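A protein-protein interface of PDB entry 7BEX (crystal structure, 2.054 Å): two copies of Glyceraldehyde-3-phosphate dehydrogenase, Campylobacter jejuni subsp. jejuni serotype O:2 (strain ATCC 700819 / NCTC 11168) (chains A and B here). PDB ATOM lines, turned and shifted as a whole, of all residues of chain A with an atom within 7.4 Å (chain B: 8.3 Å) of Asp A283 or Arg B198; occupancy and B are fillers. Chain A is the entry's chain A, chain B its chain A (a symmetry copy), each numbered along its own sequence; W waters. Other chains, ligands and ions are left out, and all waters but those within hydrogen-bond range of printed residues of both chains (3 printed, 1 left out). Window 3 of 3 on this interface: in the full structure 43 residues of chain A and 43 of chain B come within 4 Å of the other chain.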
ATOM      1  N   VAL A 238       3.340 -21.853 -12.965  1.00  0.00           N
ATOM      2  CA  VAL A 238       2.604 -20.623 -13.361  1.00  0.00           C
ATOM      3  C   VAL A 238       3.564 -19.656 -14.052  1.00  0.00           C
ATOM      4  O   VAL A 238       4.736 -19.502 -13.633  1.00  0.00           O
ATOM      5  CB  VAL A 238       1.805 -19.946 -12.229  1.00  0.00           C
ATOM      6  CG1 VAL A 238       1.067 -18.754 -12.823  1.00  0.00           C
ATOM      7  CG2 VAL A 238       0.835 -20.927 -11.566  1.00  0.00           C
ATOM      8  N   ASP A 275      -8.557 -11.198 -14.479  1.00  0.00           N
ATOM      9  CA  ASP A 275      -8.247 -10.950 -13.050  1.00  0.00           C
ATOM     10  C   ASP A 275      -8.389  -9.455 -12.787  1.00  0.00           C
ATOM     11  O   ASP A 275      -7.605  -8.666 -13.309  1.00  0.00           O
ATOM     12  CB  ASP A 275      -6.857 -11.441 -12.645  1.00  0.00           C
ATOM     13  CG  ASP A 275      -6.508 -11.123 -11.202  1.00  0.00           C
ATOM     14  OD1 ASP A 275      -7.467 -11.142 -10.375  1.00  0.00           O
ATOM     15  OD2 ASP A 275      -5.278 -10.838 -10.903  1.00  0.00           O
ATOM     16  N   ASP A 277      -8.628  -8.733  -9.386  1.00  0.00           N
ATOM     17  CA  ASP A 277      -8.296  -8.800  -7.932  1.00  0.00           C
ATOM     18  C   ASP A 277      -6.811  -8.594  -7.629  1.00  0.00           C
ATOM     19  O   ASP A 277      -6.428  -8.804  -6.436  1.00  0.00           O
ATOM     20  CB  ASP A 277      -8.691 -10.162  -7.374  1.00  0.00           C
ATOM     21  CG  ASP A 277     -10.178 -10.251  -7.049  1.00  0.00           C
ATOM     22  OD1 ASP A 277     -10.895  -9.276  -7.290  1.00  0.00           O
ATOM     23  OD2 ASP A 277     -10.563 -11.252  -6.479  1.00  0.00           O
ATOM     24  N   GLU A 278      -5.975  -8.284  -8.627  1.00  0.00           N
ATOM     25  CA  GLU A 278      -4.517  -8.070  -8.418  1.00  0.00           C
ATOM     26  C   GLU A 278      -3.890  -9.293  -7.749  1.00  0.00           C
ATOM     27  O   GLU A 278      -3.119  -9.158  -6.765  1.00  0.00           O
ATOM     28  CB  GLU A 278      -4.286  -6.786  -7.619  1.00  0.00           C
ATOM     29  CG  GLU A 278      -4.711  -5.532  -8.362  1.00  0.00           C
ATOM     30  CD  GLU A 278      -4.535  -4.293  -7.500  1.00  0.00           C
ATOM     31  OE1 GLU A 278      -3.484  -4.142  -6.923  1.00  0.00           O
ATOM     32  OE2 GLU A 278      -5.500  -3.568  -7.305  1.00  0.00           O
ATOM     33  N   ARG A 279      -4.154 -10.459  -8.316  1.00  0.00           N
ATOM     34  CA  ARG A 279      -3.496 -11.703  -7.895  1.00  0.00           C
ATOM     35  C   ARG A 279      -2.021 -11.732  -8.315  1.00  0.00           C
ATOM     36  O   ARG A 279      -1.558 -10.958  -9.203  1.00  0.00           O
ATOM     37  CB  ARG A 279      -4.299 -12.883  -8.417  1.00  0.00           C
ATOM     38  CG  ARG A 279      -5.493 -13.173  -7.527  1.00  0.00           C
ATOM     39  CD  ARG A 279      -6.406 -14.230  -8.087  1.00  0.00           C
ATOM     40  NE  ARG A 279      -7.355 -13.610  -8.996  1.00  0.00           N
ATOM     41  CZ  ARG A 279      -8.428 -14.231  -9.478  1.00  0.00           C
ATOM     42  NH1 ARG A 279      -8.636 -15.487  -9.152  1.00  0.00           N
ATOM     43  NH2 ARG A 279      -9.291 -13.619 -10.252  1.00  0.00           N
ATOM     44  N   VAL A 280      -1.298 -12.664  -7.723  1.00  0.00           N
ATOM     45  CA  VAL A 280       0.103 -12.954  -8.118  1.00  0.00           C
ATOM     46  C   VAL A 280       0.132 -14.396  -8.637  1.00  0.00           C
ATOM     47  O   VAL A 280      -0.924 -15.041  -8.640  1.00  0.00           O
ATOM     48  CB  VAL A 280       1.046 -12.682  -6.931  1.00  0.00           C
ATOM     49  CG1 VAL A 280       1.069 -11.200  -6.588  1.00  0.00           C
ATOM     50  CG2 VAL A 280       0.661 -13.494  -5.710  1.00  0.00           C
ATOM     51  N   SER A 281       1.299 -14.887  -9.052  1.00  0.00           N
ATOM     52  CA  SER A 281       1.391 -16.163  -9.812  1.00  0.00           C
ATOM     53  C   SER A 281       0.816 -17.344  -9.013  1.00  0.00           C
ATOM     54  O   SER A 281       0.074 -18.134  -9.619  1.00  0.00           O
ATOM     55  CB  SER A 281       2.821 -16.443 -10.265  1.00  0.00           C
ATOM     56  OG  SER A 281       3.684 -16.574  -9.154  1.00  0.00           O
ATOM     57  N   SER A 282       1.154 -17.499  -7.724  1.00  0.00           N
ATOM     58  CA  SER A 282       0.736 -18.665  -6.891  1.00  0.00           C
ATOM     59  C   SER A 282      -0.799 -18.766  -6.851  1.00  0.00           C
ATOM     60  O   SER A 282      -1.318 -19.854  -6.666  1.00  0.00           O
ATOM     61  CB  SER A 282       1.337 -18.639  -5.480  1.00  0.00           C
ATOM     62  OG  SER A 282       0.841 -17.541  -4.728  1.00  0.00           O
ATOM     63  N   ASP A 283      -1.497 -17.661  -7.048  1.00  0.00           N
ATOM     64  CA  ASP A 283      -2.979 -17.682  -6.954  1.00  0.00           C
ATOM     65  C   ASP A 283      -3.581 -18.436  -8.132  1.00  0.00           C
ATOM     66  O   ASP A 283      -4.799 -18.707  -8.054  1.00  0.00           O
ATOM     67  CB  ASP A 283      -3.545 -16.275  -6.940  1.00  0.00           C
ATOM     68  CG  ASP A 283      -3.059 -15.525  -5.723  1.00  0.00           C
ATOM     69  OD1 ASP A 283      -2.968 -16.201  -4.643  1.00  0.00           O
ATOM     70  OD2 ASP A 283      -2.759 -14.318  -5.850  1.00  0.00           O
ATOM     71  N   PHE A 284      -2.797 -18.759  -9.167  1.00  0.00           N
ATOM     72  CA  PHE A 284      -3.318 -19.428 -10.379  1.00  0.00           C
ATOM     73  C   PHE A 284      -2.864 -20.886 -10.431  1.00  0.00           C
ATOM     74  O   PHE A 284      -3.138 -21.561 -11.434  1.00  0.00           O
ATOM     75  CB  PHE A 284      -2.997 -18.620 -11.625  1.00  0.00           C
ATOM     76  CG  PHE A 284      -3.634 -17.264 -11.554  1.00  0.00           C
ATOM     77  CD1 PHE A 284      -5.025 -17.128 -11.653  1.00  0.00           C
ATOM     78  CD2 PHE A 284      -2.855 -16.128 -11.363  1.00  0.00           C
ATOM     79  CE1 PHE A 284      -5.634 -15.883 -11.497  1.00  0.00           C
ATOM     80  CE2 PHE A 284      -3.466 -14.881 -11.264  1.00  0.00           C
ATOM     81  CZ  PHE A 284      -4.844 -14.757 -11.295  1.00  0.00           C
ATOM     82  N   ILE A 285      -2.258 -21.364  -9.354  1.00  0.00           N
ATOM     83  CA  ILE A 285      -1.861 -22.783  -9.234  1.00  0.00           C
ATOM     84  C   ILE A 285      -3.138 -23.628  -9.254  1.00  0.00           C
ATOM     85  O   ILE A 285      -4.071 -23.344  -8.493  1.00  0.00           O
ATOM     86  CB  ILE A 285      -1.002 -23.006  -7.985  1.00  0.00           C
ATOM     87  CG1 ILE A 285       0.415 -22.449  -8.175  1.00  0.00           C
ATOM     88  CG2 ILE A 285      -0.966 -24.492  -7.671  1.00  0.00           C
ATOM     89  CD1 ILE A 285       1.243 -22.481  -6.913  1.00  0.00           C
ATOM     90  N   THR A 286      -3.224 -24.574 -10.180  1.00  0.00           N
ATOM     91  CA  THR A 286      -4.376 -25.473 -10.347  1.00  0.00           C
ATOM     92  C   THR A 286      -5.567 -24.686 -10.907  1.00  0.00           C
ATOM     93  O   THR A 286      -6.701 -25.142 -10.718  1.00  0.00           O
ATOM     94  CB  THR A 286      -4.710 -26.222  -9.039  1.00  0.00           C
ATOM     95  OG1 THR A 286      -3.490 -26.670  -8.446  1.00  0.00           O
ATOM     96  CG2 THR A 286      -5.619 -27.426  -9.255  1.00  0.00           C
ATOM     97  N   CYS A 287      -5.346 -23.615 -11.664  1.00  0.00           N
ATOM     98  CA  CYS A 287      -6.413 -22.871 -12.384  1.00  0.00           C
ATOM     99  C   CYS A 287      -6.547 -23.480 -13.783  1.00  0.00           C
ATOM    100  O   CYS A 287      -5.494 -23.716 -14.452  1.00  0.00           O
ATOM    101  CB  CYS A 287      -6.055 -21.391 -12.450  1.00  0.00           C
ATOM    102  SG  CYS A 287      -7.225 -20.376 -13.400  1.00  0.00           S
ATOM    103  N   TYR B 180      13.799  -9.623  -6.583  1.00  0.00           N
ATOM    104  CA  TYR B 180      13.047  -9.127  -5.410  1.00  0.00           C
ATOM    105  C   TYR B 180      13.933  -8.124  -4.650  1.00  0.00           C
ATOM    106  O   TYR B 180      15.164  -8.097  -4.817  1.00  0.00           O
ATOM    107  CB  TYR B 180      12.462 -10.259  -4.567  1.00  0.00           C
ATOM    108  CG  TYR B 180      13.390 -11.323  -4.055  1.00  0.00           C
ATOM    109  CD1 TYR B 180      14.330 -11.055  -3.071  1.00  0.00           C
ATOM    110  CD2 TYR B 180      13.281 -12.615  -4.517  1.00  0.00           C
ATOM    111  CE1 TYR B 180      15.168 -12.057  -2.592  1.00  0.00           C
ATOM    112  CE2 TYR B 180      14.092 -13.632  -4.036  1.00  0.00           C
ATOM    113  CZ  TYR B 180      15.023 -13.359  -3.050  1.00  0.00           C
ATOM    114  OH  TYR B 180      15.811 -14.385  -2.590  1.00  0.00           O
ATOM    115  N   GLY B 183      11.755  -3.797  -0.571  1.00  0.00           N
ATOM    116  CA  GLY B 183      10.377  -3.269  -0.624  1.00  0.00           C
ATOM    117  C   GLY B 183       9.339  -4.386  -0.596  1.00  0.00           C
ATOM    118  O   GLY B 183       8.144  -4.081  -0.535  1.00  0.00           O
ATOM    119  N   GLN B 184       9.747  -5.656  -0.644  1.00  0.00           N
ATOM    120  CA  GLN B 184       8.781  -6.768  -0.770  1.00  0.00           C
ATOM    121  C   GLN B 184       8.718  -7.572   0.540  1.00  0.00           C
ATOM    122  O   GLN B 184       9.471  -7.271   1.441  1.00  0.00           O
ATOM    123  CB  GLN B 184       9.201  -7.597  -1.970  1.00  0.00           C
ATOM    124  CG  GLN B 184       8.859  -6.960  -3.311  1.00  0.00           C
ATOM    125  CD  GLN B 184       9.270  -7.896  -4.410  1.00  0.00           C
ATOM    126  OE1 GLN B 184      10.333  -7.760  -5.003  1.00  0.00           O
ATOM    127  NE2 GLN B 184       8.436  -8.881  -4.663  1.00  0.00           N
ATOM    128  N   SER B 185       7.761  -8.481   0.686  1.00  0.00           N
ATOM    129  CA  SER B 185       7.541  -9.271   1.927  1.00  0.00           C
ATOM    130  C   SER B 185       8.105 -10.673   1.737  1.00  0.00           C
ATOM    131  O   SER B 185       7.949 -11.243   0.661  1.00  0.00           O
ATOM    132  CB  SER B 185       6.104  -9.326   2.317  1.00  0.00           C
ATOM    133  OG  SER B 185       5.449  -8.181   1.852  1.00  0.00           O
ATOM    134  N   ILE B 186       8.760 -11.204   2.762  1.00  0.00           N
ATOM    135  CA  ILE B 186       9.317 -12.583   2.731  1.00  0.00           C
ATOM    136  C   ILE B 186       8.169 -13.603   2.743  1.00  0.00           C
ATOM    137  O   ILE B 186       8.240 -14.602   1.993  1.00  0.00           O
ATOM    138  CB  ILE B 186      10.365 -12.770   3.840  1.00  0.00           C
ATOM    139  CG1 ILE B 186      11.000 -14.156   3.786  1.00  0.00           C
ATOM    140  CG2 ILE B 186       9.799 -12.459   5.202  1.00  0.00           C
ATOM    141  CD1 ILE B 186      11.712 -14.474   2.471  1.00  0.00           C
ATOM    142  N   ILE B 187       7.115 -13.336   3.510  1.00  0.00           N
ATOM    143  CA  ILE B 187       5.883 -14.172   3.564  1.00  0.00           C
ATOM    144  C   ILE B 187       4.693 -13.226   3.350  1.00  0.00           C
ATOM    145  O   ILE B 187       4.921 -11.994   3.333  1.00  0.00           O
ATOM    146  CB  ILE B 187       5.791 -14.982   4.878  1.00  0.00           C
ATOM    147  CG1 ILE B 187       5.900 -14.122   6.144  1.00  0.00           C
ATOM    148  CG2 ILE B 187       6.858 -16.080   4.899  1.00  0.00           C
ATOM    149  CD1 ILE B 187       4.832 -13.063   6.340  1.00  0.00           C
ATOM    150  N   ASP B 188       3.511 -13.753   3.050  1.00  0.00           N
ATOM    151  CA  ASP B 188       2.297 -12.925   2.830  1.00  0.00           C
ATOM    152  C   ASP B 188       2.040 -12.099   4.099  1.00  0.00           C
ATOM    153  O   ASP B 188       1.698 -12.721   5.165  1.00  0.00           O
ATOM    154  CB  ASP B 188       1.069 -13.768   2.484  1.00  0.00           C
ATOM    155  CG  ASP B 188       1.081 -14.516   1.155  1.00  0.00           C
ATOM    156  OD1 ASP B 188       2.057 -14.449   0.360  1.00  0.00           O
ATOM    157  OD2 ASP B 188       0.075 -15.177   0.918  1.00  0.00           O
ATOM    158  N   ALA B 189       2.265 -10.772   4.016  1.00  0.00           N
ATOM    159  CA  ALA B 189       2.149  -9.864   5.179  1.00  0.00           C
ATOM    160  C   ALA B 189       1.926  -8.451   4.679  1.00  0.00           C
ATOM    161  O   ALA B 189       2.325  -8.167   3.561  1.00  0.00           O
ATOM    162  CB  ALA B 189       3.391  -9.951   6.023  1.00  0.00           C
ATOM    163  N   LYS B 190       1.382  -7.606   5.547  1.00  0.00           N
ATOM    164  CA  LYS B 190       1.065  -6.185   5.266  1.00  0.00           C
ATOM    165  C   LYS B 190       2.265  -5.500   4.594  1.00  0.00           C
ATOM    166  O   LYS B 190       3.357  -5.588   5.101  1.00  0.00           O
ATOM    167  CB  LYS B 190       0.710  -5.463   6.567  1.00  0.00           C
ATOM    168  CG  LYS B 190       0.532  -3.960   6.390  1.00  0.00           C
ATOM    169  CD  LYS B 190       0.504  -3.240   7.728  1.00  0.00           C
ATOM    170  CE  LYS B 190       0.126  -1.781   7.651  1.00  0.00           C
ATOM    171  NZ  LYS B 190       0.184  -1.221   9.023  1.00  0.00           N
ATOM    172  N   ALA B 191       2.052  -4.875   3.440  1.00  0.00           N
ATOM    173  CA  ALA B 191       3.004  -3.966   2.789  1.00  0.00           C
ATOM    174  C   ALA B 191       2.193  -2.808   2.214  1.00  0.00           C
ATOM    175  O   ALA B 191       0.980  -2.737   2.462  1.00  0.00           O
ATOM    176  CB  ALA B 191       3.778  -4.696   1.723  1.00  0.00           C
ATOM    177  N   ASP B 193       1.073  -2.059  -0.646  1.00  0.00           N
ATOM    178  CA  ASP B 193       0.010  -2.415  -1.630  1.00  0.00           C
ATOM    179  C   ASP B 193      -0.207  -3.935  -1.608  1.00  0.00           C
ATOM    180  O   ASP B 193       0.566  -4.697  -0.952  1.00  0.00           O
ATOM    181  CB  ASP B 193       0.333  -1.866  -3.035  1.00  0.00           C
ATOM    182  CG  ASP B 193       1.599  -2.453  -3.643  1.00  0.00           C
ATOM    183  OD1 ASP B 193       1.552  -3.615  -4.124  1.00  0.00           O
ATOM    184  OD2 ASP B 193       2.644  -1.766  -3.596  1.00  0.00           O
ATOM    185  N   LYS B 194      -1.267  -4.353  -2.274  1.00  0.00           N
ATOM    186  CA  LYS B 194      -1.711  -5.751  -2.330  1.00  0.00           C
ATOM    187  C   LYS B 194      -0.556  -6.615  -2.809  1.00  0.00           C
ATOM    188  O   LYS B 194      -0.148  -7.471  -2.032  1.00  0.00           O
ATOM    189  CB  LYS B 194      -2.925  -5.881  -3.232  1.00  0.00           C
ATOM    190  CG  LYS B 194      -4.192  -5.363  -2.589  1.00  0.00           C
ATOM    191  CD  LYS B 194      -5.334  -5.349  -3.576  1.00  0.00           C
ATOM    192  CE  LYS B 194      -6.576  -4.733  -2.979  1.00  0.00           C
ATOM    193  NZ  LYS B 194      -7.730  -4.965  -3.878  1.00  0.00           N
ATOM    194  N   ARG B 195      -0.063  -6.378  -4.029  1.00  0.00           N
ATOM    195  CA  ARG B 195       0.900  -7.327  -4.674  1.00  0.00           C
ATOM    196  C   ARG B 195       2.225  -7.373  -3.878  1.00  0.00           C
ATOM    197  O   ARG B 195       2.786  -8.495  -3.614  1.00  0.00           O
ATOM    198  CB  ARG B 195       1.022  -6.970  -6.163  1.00  0.00           C
ATOM    199  CG  ARG B 195      -0.213  -7.352  -6.976  1.00  0.00           C
ATOM    200  CD  ARG B 195       0.205  -7.745  -8.376  1.00  0.00           C
ATOM    201  NE  ARG B 195      -0.845  -8.005  -9.342  1.00  0.00           N
ATOM    202  CZ  ARG B 195      -1.433  -7.089 -10.112  1.00  0.00           C
ATOM    203  NH1 ARG B 195      -1.209  -5.789  -9.967  1.00  0.00           N
ATOM    204  NH2 ARG B 195      -2.322  -7.483 -10.992  1.00  0.00           N
ATOM    205  N   ARG B 196       2.710  -6.236  -3.400  1.00  0.00           N
ATOM    206  CA  ARG B 196       3.966  -6.220  -2.593  1.00  0.00           C
ATOM    207  C   ARG B 196       3.785  -6.958  -1.256  1.00  0.00           C
ATOM    208  O   ARG B 196       4.818  -7.246  -0.627  1.00  0.00           O
ATOM    209  CB  ARG B 196       4.431  -4.807  -2.238  1.00  0.00           C
ATOM    210  CG  ARG B 196       5.287  -4.178  -3.312  1.00  0.00           C
ATOM    211  CD  ARG B 196       5.265  -2.673  -3.125  1.00  0.00           C
ATOM    212  NE  ARG B 196       5.704  -1.998  -4.341  1.00  0.00           N
ATOM    213  CZ  ARG B 196       6.960  -1.974  -4.724  1.00  0.00           C
ATOM    214  NH1 ARG B 196       7.864  -2.620  -4.000  1.00  0.00           N
ATOM    215  NH2 ARG B 196       7.308  -1.347  -5.839  1.00  0.00           N
ATOM    216  N   SER B 197       2.549  -7.227  -0.821  1.00  0.00           N
ATOM    217  CA  SER B 197       2.280  -7.956   0.455  1.00  0.00           C
ATOM    218  C   SER B 197       2.556  -9.457   0.275  1.00  0.00           C
ATOM    219  O   SER B 197       2.528 -10.153   1.296  1.00  0.00           O
ATOM    220  CB  SER B 197       0.862  -7.701   0.947  1.00  0.00           C
ATOM    221  OG  SER B 197       0.644  -6.315   1.209  1.00  0.00           O
ATOM    222  N   ARG B 198       2.816  -9.935  -0.962  1.00  0.00           N
ATOM    223  CA  ARG B 198       2.880 -11.389  -1.258  1.00  0.00           C
ATOM    224  C   ARG B 198       4.326 -11.895  -1.264  1.00  0.00           C
ATOM    225  O   ARG B 198       5.259 -11.119  -1.517  1.00  0.00           O
ATOM    226  CB  ARG B 198       2.106 -11.699  -2.542  1.00  0.00           C
ATOM    227  CG  ARG B 198       0.652 -11.221  -2.517  1.00  0.00           C
ATOM    228  CD  ARG B 198      -0.215 -11.871  -1.451  1.00  0.00           C
ATOM    229  NE  ARG B 198      -0.327 -13.296  -1.701  1.00  0.00           N
ATOM    230  CZ  ARG B 198      -1.062 -13.837  -2.664  1.00  0.00           C
ATOM    231  NH1 ARG B 198      -1.862 -13.074  -3.377  1.00  0.00           N
ATOM    232  NH2 ARG B 198      -1.033 -15.152  -2.876  1.00  0.00           N
ATOM    233  N   ALA B 199       4.488 -13.124  -0.806  1.00  0.00           N
ATOM    234  CA  ALA B 199       5.782 -13.792  -0.585  1.00  0.00           C
ATOM    235  C   ALA B 199       6.674 -13.655  -1.839  1.00  0.00           C
ATOM    236  O   ALA B 199       6.376 -14.199  -2.897  1.00  0.00           O
ATOM    237  CB  ALA B 199       5.519 -15.219  -0.222  1.00  0.00           C
ATOM    238  N   ALA B 200       7.765 -12.915  -1.709  1.00  0.00           N
ATOM    239  CA  ALA B 200       8.602 -12.489  -2.850  1.00  0.00           C
ATOM    240  C   ALA B 200       9.383 -13.644  -3.484  1.00  0.00           C
ATOM    241  O   ALA B 200       9.699 -13.558  -4.708  1.00  0.00           O
ATOM    242  CB  ALA B 200       9.511 -11.402  -2.353  1.00  0.00           C
ATOM    243  N   ALA B 201       9.810 -14.639  -2.709  1.00  0.00           N
ATOM    244  CA  ALA B 201      10.679 -15.717  -3.236  1.00  0.00           C
ATOM    245  C   ALA B 201       9.842 -16.909  -3.745  1.00  0.00           C
ATOM    246  O   ALA B 201      10.450 -17.925  -4.182  1.00  0.00           O
ATOM    247  CB  ALA B 201      11.673 -16.110  -2.170  1.00  0.00           C
ATOM    248  N   GLN B 202       8.496 -16.774  -3.765  1.00  0.00           N
ATOM    249  CA  GLN B 202       7.585 -17.878  -4.159  1.00  0.00           C
ATOM    250  C   GLN B 202       6.530 -17.383  -5.162  1.00  0.00           C
ATOM    251  O   GLN B 202       5.534 -18.060  -5.342  1.00  0.00           O
ATOM    252  CB  GLN B 202       6.911 -18.453  -2.912  1.00  0.00           C
ATOM    253  CG  GLN B 202       7.892 -19.197  -2.044  1.00  0.00           C
ATOM    254  CD  GLN B 202       8.268 -20.550  -2.608  1.00  0.00           C
ATOM    255  OE1 GLN B 202       9.438 -20.808  -2.985  1.00  0.00           O
ATOM    256  NE2 GLN B 202       7.248 -21.391  -2.687  1.00  0.00           N
ATOM    257  N   ASN B 203       6.743 -16.238  -5.806  1.00  0.00           N
ATOM    258  CA  ASN B 203       5.752 -15.679  -6.746  1.00  0.00           C
ATOM    259  C   ASN B 203       6.446 -14.868  -7.844  1.00  0.00           C
ATOM    260  O   ASN B 203       7.494 -14.264  -7.551  1.00  0.00           O
ATOM    261  CB  ASN B 203       4.815 -14.726  -6.008  1.00  0.00           C
ATOM    262  CG  ASN B 203       3.787 -15.413  -5.140  1.00  0.00           C
ATOM    263  OD1 ASN B 203       2.931 -16.159  -5.645  1.00  0.00           O
ATOM    264  ND2 ASN B 203       3.881 -15.173  -3.844  1.00  0.00           N
ATOM    265  N   ILE B 204       5.826 -14.799  -9.019  1.00  0.00           N
ATOM    266  CA  ILE B 204       5.976 -13.647  -9.948  1.00  0.00           C
ATOM    267  C   ILE B 204       5.012 -12.535  -9.506  1.00  0.00           C
ATOM    268  O   ILE B 204       3.789 -12.808  -9.375  1.00  0.00           O
ATOM    269  CB  ILE B 204       5.701 -14.087 -11.385  1.00  0.00           C
ATOM    270  CG1 ILE B 204       6.575 -15.268 -11.796  1.00  0.00           C
ATOM    271  CG2 ILE B 204       5.844 -12.921 -12.331  1.00  0.00           C
ATOM    272  CD1 ILE B 204       6.051 -15.999 -13.030  1.00  0.00           C
ATOM    273  N   ILE B 205       5.527 -11.331  -9.273  1.00  0.00           N
ATOM    274  CA  ILE B 205       4.763 -10.226  -8.620  1.00  0.00           C
ATOM    275  C   ILE B 205       4.841  -8.981  -9.500  1.00  0.00           C
ATOM    276  O   ILE B 205       5.842  -8.286  -9.530  1.00  0.00           O
ATOM    277  CB  ILE B 205       5.260  -9.979  -7.193  1.00  0.00           C
ATOM    278  CG1 ILE B 205       5.159 -11.251  -6.339  1.00  0.00           C
ATOM    279  CG2 ILE B 205       4.560  -8.796  -6.558  1.00  0.00           C
ATOM    280  CD1 ILE B 205       5.365 -11.016  -4.873  1.00  0.00           C
ATOM    281  N   PRO B 206       3.777  -8.680 -10.258  1.00  0.00           N
ATOM    282  CA  PRO B 206       3.691  -7.396 -10.951  1.00  0.00           C
ATOM    283  C   PRO B 206       3.858  -6.248  -9.944  1.00  0.00           C
ATOM    284  O   PRO B 206       3.206  -6.264  -8.881  1.00  0.00           O
ATOM    285  CB  PRO B 206       2.284  -7.388 -11.534  1.00  0.00           C
ATOM    286  CG  PRO B 206       1.907  -8.855 -11.656  1.00  0.00           C
ATOM    287  CD  PRO B 206       2.593  -9.527 -10.472  1.00  0.00           C
ATOM    288  N   ARG B 232       8.396  -8.816 -10.652  1.00  0.00           N
ATOM    289  CA  ARG B 232       9.376  -9.243  -9.635  1.00  0.00           C
ATOM    290  C   ARG B 232       9.351 -10.763  -9.573  1.00  0.00           C
ATOM    291  O   ARG B 232       8.245 -11.330  -9.496  1.00  0.00           O
ATOM    292  CB  ARG B 232       9.048  -8.637  -8.269  1.00  0.00           C
ATOM    293  CG  ARG B 232       9.092  -7.125  -8.241  1.00  0.00           C
ATOM    294  CD  ARG B 232      10.501  -6.606  -8.315  1.00  0.00           C
ATOM    295  NE  ARG B 232      10.570  -5.154  -8.252  1.00  0.00           N
ATOM    296  CZ  ARG B 232      10.717  -4.428  -7.155  1.00  0.00           C
ATOM    297  NH1 ARG B 232      10.747  -4.972  -5.950  1.00  0.00           N
ATOM    298  NH2 ARG B 232      10.778  -3.121  -7.269  1.00  0.00           N
HETATM  299  O   HOH W   1      -2.785 -10.449 -11.507  1.00  0.00           O
HETATM  300  O   HOH W   2      -8.248  -7.634  -4.766  1.00  0.00           O
HETATM  301  O   HOH W   3      -0.692  -4.140  -5.656  1.00  0.00           O
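Asp A283 touches just one residue of chain B: Arg B198. Printed residues of chain A within 4 Å of Arg B198: Val A280 (3.5 Å), Ser A282 (3.6 Å) and Asp A283 (2.8 Å). Of the printed residues of chain B, Arg A279 touches Arg B195 (3.0 Å). Printed residues of chain A within 4 Å of Ile B204: Val A238 (3.8 Å), Val A280 (3.7 Å) and Ser A281 (2.8 Å). The nearest printed residue of chain B that does not touch Arg A279 is Pro B206 (4.6 Å).
OD1 of Asp A275 is in salt-bridge range of NE of Arg A279. The side-chain carboxylate (OD1) of Asp B193 sits at hydrogen-bond distance from the backbone NH (N) of Arg B195 (3.2 Å). The backbone carbonyl oxygen (O) of Ala B199 sits at hydrogen-bond distance from the side-chain amide nitrogen (ND2) of Asn B203, 2.8 Å away. The side-chain carboxylate (OD2) of Asp B188 is in salt-bridge range of the guanidinium group (NE) of Arg B198. The backbone NH (N) of Val A280 is in hydrogen-bond range of the side-chain carboxylate (OD2) of Asp A283, at 2.9 Å. OD2 of Asp A275 lies within hydrogen-bond range of N of Glu A278 (3.5 Å).
Of the 13 printed residues of chain A, 7 touch a printed residue of chain B. Printed residues of chain A that touch a printed residue of chain B: Val A238, Glu A278, Arg A279, Val A280, Ser A281, Ser A282 and Asp A283. Hydrophobic or aromatic side chains of chain A within 4 Å of the printed part of chain B: Val A280. Of the 25 printed residues of chain B, 4 touch a printed residue of chain A. Hydrophobic or aromatic side chains of chain B within 4 Å of the printed part of chain A: Ile B204. Among the printed residues, 12 pairs touch across the chains. Among the printed residues, Asp or Glu carboxylates within 4 Å of a Lys or Arg side-chain nitrogen of the other chain: Asp A283 with Arg B198.
The side-chain hydroxyl (OG) of Ser A282 is in hydrogen-bond range of the side-chain amide oxygen (OD1) of Asn B203 (2.7 Å). The guanidinium group (NH2) of Arg B198 is in salt-bridge range of the side-chain carboxylate (OD1) of Asp A283. The side-chain hydroxyl (OG) of Ser A281 lies within hydrogen-bond range of the backbone NH (N) of Ile B204, at 2.8 Å. O of Arg A279 sits at hydrogen-bond distance from NE of Arg B195 (3.0 Å).
Water W1 lies within hydrogen-bond range of the side-chain carboxylate of Asp A275 (2.6 Å), the backbone carbonyl oxygen of Arg A279 (2.7 Å) and the guanidinium group of Arg B195 (3.0 Å). Water W2 lies within hydrogen-bond range of the backbone carbonyl oxygen of Asp A277 and the side-chain amino group of Lys B194. Water W3 lies within hydrogen-bond range of the side-chain carboxylate (OD1) of Asp B193, the backbone NH (N) of Arg B195, the side-chain carboxylate (OE1) of Glu A278 and the backbone NH (N) of Lys B194.
No position is printed for both chains.
Among the printed residues, pairs that only touch across the chains: Ser A281 with Asn B203 (3.3 Å), Glu A278 with Arg B195 (3.4 Å), Val A280 with Arg B198 (3.5 Å), Val A280 with Asn B203 (3.5 Å), Ser A282 with Arg B198 (3.6 Å), Val A280 with Ile B204 (3.7 Å), Val A238 with Ile B204 (3.8 Å) and Val A280 with Arg B195 (3.99 Å).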
